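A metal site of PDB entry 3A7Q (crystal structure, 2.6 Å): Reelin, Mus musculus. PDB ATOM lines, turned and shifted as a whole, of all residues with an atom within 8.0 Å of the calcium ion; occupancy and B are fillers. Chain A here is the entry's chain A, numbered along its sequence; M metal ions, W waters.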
ATOM      1  N   ASP A 576      26.940 -21.889  -9.536  1.00  0.00           N
ATOM      2  CA  ASP A 576      26.263 -20.601  -9.803  1.00  0.00           C
ATOM      3  C   ASP A 576      26.048 -19.725  -8.564  1.00  0.00           C
ATOM      4  O   ASP A 576      25.428 -20.139  -7.570  1.00  0.00           O
ATOM      5  CB  ASP A 576      24.940 -20.799 -10.578  1.00  0.00           C
ATOM      6  CG  ASP A 576      24.536 -19.545 -11.386  1.00  0.00           C
ATOM      7  OD1 ASP A 576      24.960 -18.406 -11.050  1.00  0.00           O
ATOM      8  OD2 ASP A 576      23.775 -19.705 -12.370  1.00  0.00           O
ATOM      9  N   ASN A 577      26.591 -18.522  -8.631  1.00  0.00           N
ATOM     10  CA  ASN A 577      26.539 -17.541  -7.559  1.00  0.00           C
ATOM     11  C   ASN A 577      25.334 -16.592  -7.675  1.00  0.00           C
ATOM     12  O   ASN A 577      24.941 -15.951  -6.700  1.00  0.00           O
ATOM     13  CB  ASN A 577      27.847 -16.752  -7.471  1.00  0.00           C
ATOM     14  CG  ASN A 577      28.559 -16.564  -8.847  1.00  0.00           C
ATOM     15  OD1 ASN A 577      28.186 -17.171  -9.862  1.00  0.00           O
ATOM     16  ND2 ASN A 577      29.597 -15.730  -8.856  1.00  0.00           N
ATOM     17  N   PHE A 578      24.741 -16.542  -8.867  1.00  0.00           N
ATOM     18  CA  PHE A 578      23.666 -15.600  -9.206  1.00  0.00           C
ATOM     19  C   PHE A 578      24.067 -14.136  -8.962  1.00  0.00           C
ATOM     20  O   PHE A 578      23.276 -13.324  -8.484  1.00  0.00           O
ATOM     21  CB  PHE A 578      22.352 -15.956  -8.503  1.00  0.00           C
ATOM     22  CG  PHE A 578      21.937 -17.409  -8.661  1.00  0.00           C
ATOM     23  CD1 PHE A 578      21.608 -17.941  -9.901  1.00  0.00           C
ATOM     24  CD2 PHE A 578      21.869 -18.246  -7.547  1.00  0.00           C
ATOM     25  CE1 PHE A 578      21.218 -19.283 -10.033  1.00  0.00           C
ATOM     26  CE2 PHE A 578      21.491 -19.584  -7.671  1.00  0.00           C
ATOM     27  CZ  PHE A 578      21.165 -20.103  -8.914  1.00  0.00           C
ATOM     28  N   ASN A 579      25.312 -13.797  -9.290  1.00  0.00           N
ATOM     29  CA  ASN A 579      25.736 -12.402  -9.224  1.00  0.00           C
ATOM     30  C   ASN A 579      25.614 -11.772 -10.603  1.00  0.00           C
ATOM     31  O   ASN A 579      25.691 -10.560 -10.749  1.00  0.00           O
ATOM     32  CB  ASN A 579      27.153 -12.283  -8.637  1.00  0.00           C
ATOM     33  CG  ASN A 579      27.291 -12.982  -7.278  1.00  0.00           C
ATOM     34  OD1 ASN A 579      26.294 -13.160  -6.542  1.00  0.00           O
ATOM     35  ND2 ASN A 579      28.511 -13.383  -6.939  1.00  0.00           N
ATOM     36  N   ARG A 580      25.412 -12.632 -11.603  1.00  0.00           N
ATOM     37  CA  ARG A 580      25.204 -12.240 -12.991  1.00  0.00           C
ATOM     38  C   ARG A 580      23.984 -12.987 -13.543  1.00  0.00           C
ATOM     39  O   ARG A 580      23.392 -13.804 -12.817  1.00  0.00           O
ATOM     40  CB  ARG A 580      26.458 -12.556 -13.812  1.00  0.00           C
ATOM     41  CG  ARG A 580      27.578 -11.552 -13.596  1.00  0.00           C
ATOM     42  CD  ARG A 580      28.968 -12.182 -13.504  1.00  0.00           C
ATOM     43  NE  ARG A 580      29.314 -13.012 -14.658  1.00  0.00           N
ATOM     44  CZ  ARG A 580      29.269 -14.345 -14.667  1.00  0.00           C
ATOM     45  NH1 ARG A 580      28.875 -15.001 -13.581  1.00  0.00           N
ATOM     46  NH2 ARG A 580      29.593 -15.012 -15.755  1.00  0.00           N
ATOM     47  N   LEU A 595      16.588 -12.446 -10.733  1.00  0.00           N
ATOM     48  CA  LEU A 595      17.555 -11.880  -9.796  1.00  0.00           C
ATOM     49  C   LEU A 595      16.932 -10.754  -8.962  1.00  0.00           C
ATOM     50  O   LEU A 595      16.285  -9.856  -9.509  1.00  0.00           O
ATOM     51  CB  LEU A 595      18.798 -11.378 -10.542  1.00  0.00           C
ATOM     52  CG  LEU A 595      19.591 -12.381 -11.380  1.00  0.00           C
ATOM     53  CD1 LEU A 595      20.842 -11.718 -11.964  1.00  0.00           C
ATOM     54  CD2 LEU A 595      19.987 -13.594 -10.572  1.00  0.00           C
ATOM     55  N   SER A 596      17.130 -10.838  -7.648  1.00  0.00           N
ATOM     56  CA  SER A 596      16.557  -9.870  -6.712  1.00  0.00           C
ATOM     57  C   SER A 596      17.432  -9.682  -5.470  1.00  0.00           C
ATOM     58  O   SER A 596      18.359 -10.467  -5.217  1.00  0.00           O
ATOM     59  CB  SER A 596      15.160 -10.316  -6.302  1.00  0.00           C
ATOM     60  OG  SER A 596      14.578  -9.396  -5.391  1.00  0.00           O
ATOM     61  N   GLY A 600      17.347 -10.209   0.992  1.00  0.00           N
ATOM     62  CA  GLY A 600      18.603  -9.891   1.630  1.00  0.00           C
ATOM     63  C   GLY A 600      19.623 -10.895   1.146  1.00  0.00           C
ATOM     64  O   GLY A 600      19.417 -11.568   0.121  1.00  0.00           O
ATOM     65  N   ALA A 601      20.720 -11.020   1.883  1.00  0.00           N
ATOM     66  CA  ALA A 601      21.729 -12.005   1.577  1.00  0.00           C
ATOM     67  C   ALA A 601      21.215 -13.396   1.931  1.00  0.00           C
ATOM     68  O   ALA A 601      20.919 -13.691   3.107  1.00  0.00           O
ATOM     69  CB  ALA A 601      23.013 -11.691   2.332  1.00  0.00           C
ATOM     70  N   VAL A 602      21.054 -14.236   0.907  1.00  0.00           N
ATOM     71  CA  VAL A 602      20.688 -15.628   1.106  1.00  0.00           C
ATOM     72  C   VAL A 602      22.000 -16.396   1.251  1.00  0.00           C
ATOM     73  O   VAL A 602      22.204 -17.080   2.257  1.00  0.00           O
ATOM     74  CB  VAL A 602      19.766 -16.165  -0.013  1.00  0.00           C
ATOM     75  CG1 VAL A 602      19.676 -17.686   0.026  1.00  0.00           C
ATOM     76  CG2 VAL A 602      18.371 -15.548   0.116  1.00  0.00           C
ATOM     77  N   ALA A 603      22.875 -16.251   0.259  1.00  0.00           N
ATOM     78  CA  ALA A 603      24.291 -16.532   0.452  1.00  0.00           C
ATOM     79  C   ALA A 603      25.006 -15.186   0.452  1.00  0.00           C
ATOM     80  O   ALA A 603      25.523 -14.755   1.472  1.00  0.00           O
ATOM     81  CB  ALA A 603      24.830 -17.430  -0.635  1.00  0.00           C
ATOM     82  N   SER A 604      25.007 -14.521  -0.703  1.00  0.00           N
ATOM     83  CA  SER A 604      25.620 -13.215  -0.869  1.00  0.00           C
ATOM     84  C   SER A 604      25.114 -12.623  -2.170  1.00  0.00           C
ATOM     85  O   SER A 604      24.568 -13.352  -3.003  1.00  0.00           O
ATOM     86  CB  SER A 604      27.153 -13.309  -0.900  1.00  0.00           C
ATOM     87  OG  SER A 604      27.584 -14.137  -1.964  1.00  0.00           O
ATOM     88  N   GLY A 605      25.283 -11.301  -2.330  1.00  0.00           N
ATOM     89  CA  GLY A 605      24.786 -10.568  -3.498  1.00  0.00           C
ATOM     90  C   GLY A 605      23.328 -10.829  -3.845  1.00  0.00           C
ATOM     91  O   GLY A 605      22.470 -10.894  -2.969  1.00  0.00           O
ATOM     92  N   LEU A 606      23.076 -11.002  -5.135  1.00  0.00           N
ATOM     93  CA  LEU A 606      21.763 -11.364  -5.650  1.00  0.00           C
ATOM     94  C   LEU A 606      21.512 -12.874  -5.557  1.00  0.00           C
ATOM     95  O   LEU A 606      22.427 -13.670  -5.654  1.00  0.00           O
ATOM     96  CB  LEU A 606      21.636 -10.920  -7.106  1.00  0.00           C
ATOM     97  CG  LEU A 606      21.673  -9.411  -7.369  1.00  0.00           C
ATOM     98  CD1 LEU A 606      22.466  -9.103  -8.631  1.00  0.00           C
ATOM     99  CD2 LEU A 606      20.258  -8.848  -7.459  1.00  0.00           C
ATOM    100  N   ALA A 607      20.261 -13.233  -5.319  1.00  0.00           N
ATOM    101  CA  ALA A 607      19.830 -14.612  -5.342  1.00  0.00           C
ATOM    102  C   ALA A 607      18.825 -14.732  -6.491  1.00  0.00           C
ATOM    103  O   ALA A 607      18.322 -13.726  -7.003  1.00  0.00           O
ATOM    104  CB  ALA A 607      19.183 -14.990  -3.979  1.00  0.00           C
ATOM    105  N   LEU A 608      18.551 -15.952  -6.914  1.00  0.00           N
ATOM    106  CA  LEU A 608      17.508 -16.198  -7.897  1.00  0.00           C
ATOM    107  C   LEU A 608      16.201 -16.312  -7.132  1.00  0.00           C
ATOM    108  O   LEU A 608      15.960 -17.277  -6.397  1.00  0.00           O
ATOM    109  CB  LEU A 608      17.813 -17.450  -8.726  1.00  0.00           C
ATOM    110  CG  LEU A 608      16.869 -17.941  -9.842  1.00  0.00           C
ATOM    111  CD1 LEU A 608      16.459 -16.856 -10.854  1.00  0.00           C
ATOM    112  CD2 LEU A 608      17.497 -19.160 -10.545  1.00  0.00           C
ATOM    113  N   ILE A 711      17.038 -19.159  -3.989  1.00  0.00           N
ATOM    114  CA  ILE A 711      18.148 -20.079  -3.985  1.00  0.00           C
ATOM    115  C   ILE A 711      19.430 -19.324  -4.366  1.00  0.00           C
ATOM    116  O   ILE A 711      19.450 -18.550  -5.326  1.00  0.00           O
ATOM    117  CB  ILE A 711      17.876 -21.247  -4.984  1.00  0.00           C
ATOM    118  CG1 ILE A 711      18.882 -22.378  -4.820  1.00  0.00           C
ATOM    119  CG2 ILE A 711      17.844 -20.758  -6.470  1.00  0.00           C
ATOM    120  CD1 ILE A 711      18.426 -23.637  -5.480  1.00  0.00           C
ATOM    121  N   ASP A 712      20.492 -19.522  -3.593  1.00  0.00           N
ATOM    122  CA  ASP A 712      21.773 -18.881  -3.892  1.00  0.00           C
ATOM    123  C   ASP A 712      22.899 -19.898  -3.801  1.00  0.00           C
ATOM    124  O   ASP A 712      22.768 -20.930  -3.113  1.00  0.00           O
ATOM    125  CB  ASP A 712      22.029 -17.683  -2.974  1.00  0.00           C
ATOM    126  CG  ASP A 712      22.950 -16.630  -3.612  1.00  0.00           C
ATOM    127  OD1 ASP A 712      23.166 -15.566  -3.026  1.00  0.00           O
ATOM    128  OD2 ASP A 712      23.473 -16.851  -4.707  1.00  0.00           O
ATOM    129  N   ASN A 713      24.008 -19.604  -4.484  1.00  0.00           N
ATOM    130  CA  ASN A 713      25.224 -20.402  -4.393  1.00  0.00           C
ATOM    131  C   ASN A 713      24.985 -21.882  -4.587  1.00  0.00           C
ATOM    132  O   ASN A 713      25.193 -22.691  -3.686  1.00  0.00           O
ATOM    133  CB  ASN A 713      25.955 -20.152  -3.075  1.00  0.00           C
ATOM    134  CG  ASN A 713      26.907 -18.958  -3.139  1.00  0.00           C
ATOM    135  OD1 ASN A 713      26.568 -17.897  -3.669  1.00  0.00           O
ATOM    136  ND2 ASN A 713      28.085 -19.125  -2.577  1.00  0.00           N
ATOM    137  N   VAL A 714      24.527 -22.233  -5.775  1.00  0.00           N
ATOM    138  CA  VAL A 714      24.316 -23.603  -6.151  1.00  0.00           C
ATOM    139  C   VAL A 714      25.662 -24.208  -6.527  1.00  0.00           C
ATOM    140  O   VAL A 714      26.454 -23.585  -7.242  1.00  0.00           O
ATOM    141  CB  VAL A 714      23.300 -23.706  -7.309  1.00  0.00           C
ATOM    142  CG1 VAL A 714      23.144 -25.156  -7.777  1.00  0.00           C
ATOM    143  CG2 VAL A 714      21.941 -23.133  -6.874  1.00  0.00           C
HETATM  144 CA    CA M   1      24.401 -14.716  -4.848  1.00  0.00          CA
HETATM  145  O   HOH W   1      26.337 -15.408  -3.768  1.00  0.00           O
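The backbone NH of Ala 603 sits close to the side-chain carboxylate of Asp 712 (3.4 Å).
The side-chain amide nitrogen (ND2) of Asn 577 sits close to the side-chain amide nitrogen (ND2) of Asn 579.
The side-chain carboxylate of Asp 712 sits close to the side-chain amide oxygen of Asn 713 (3.4 Å).
Within 4 Å of the calcium ion: Asn 577, Asn 579, Ser 604, Leu 606 and Asp 712.
The nearest printed residue that does not touch the calcium ion is Asn 713 (4.03 Å).
The calcium ion is bound by the backbone carbonyl oxygen (O) of Asn 577, the backbone carbonyl oxygen (O) of Ser 604, water W1, the side-chain carboxylate (OD2) of Asp 712, the side-chain carboxylate (OD1) of Asp 712 and the backbone carbonyl oxygen (O) of Leu 606.
The calcium ion has six donor atoms within binding distance.
Slightly farther from the calcium ion lies OD1 of Asn 579 (3.0 Å).
Water W1 bridges the side-chain amide oxygen of Asn 713 (2.5 Å) and the side-chain hydroxyl of Ser 604 (2.5 Å).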
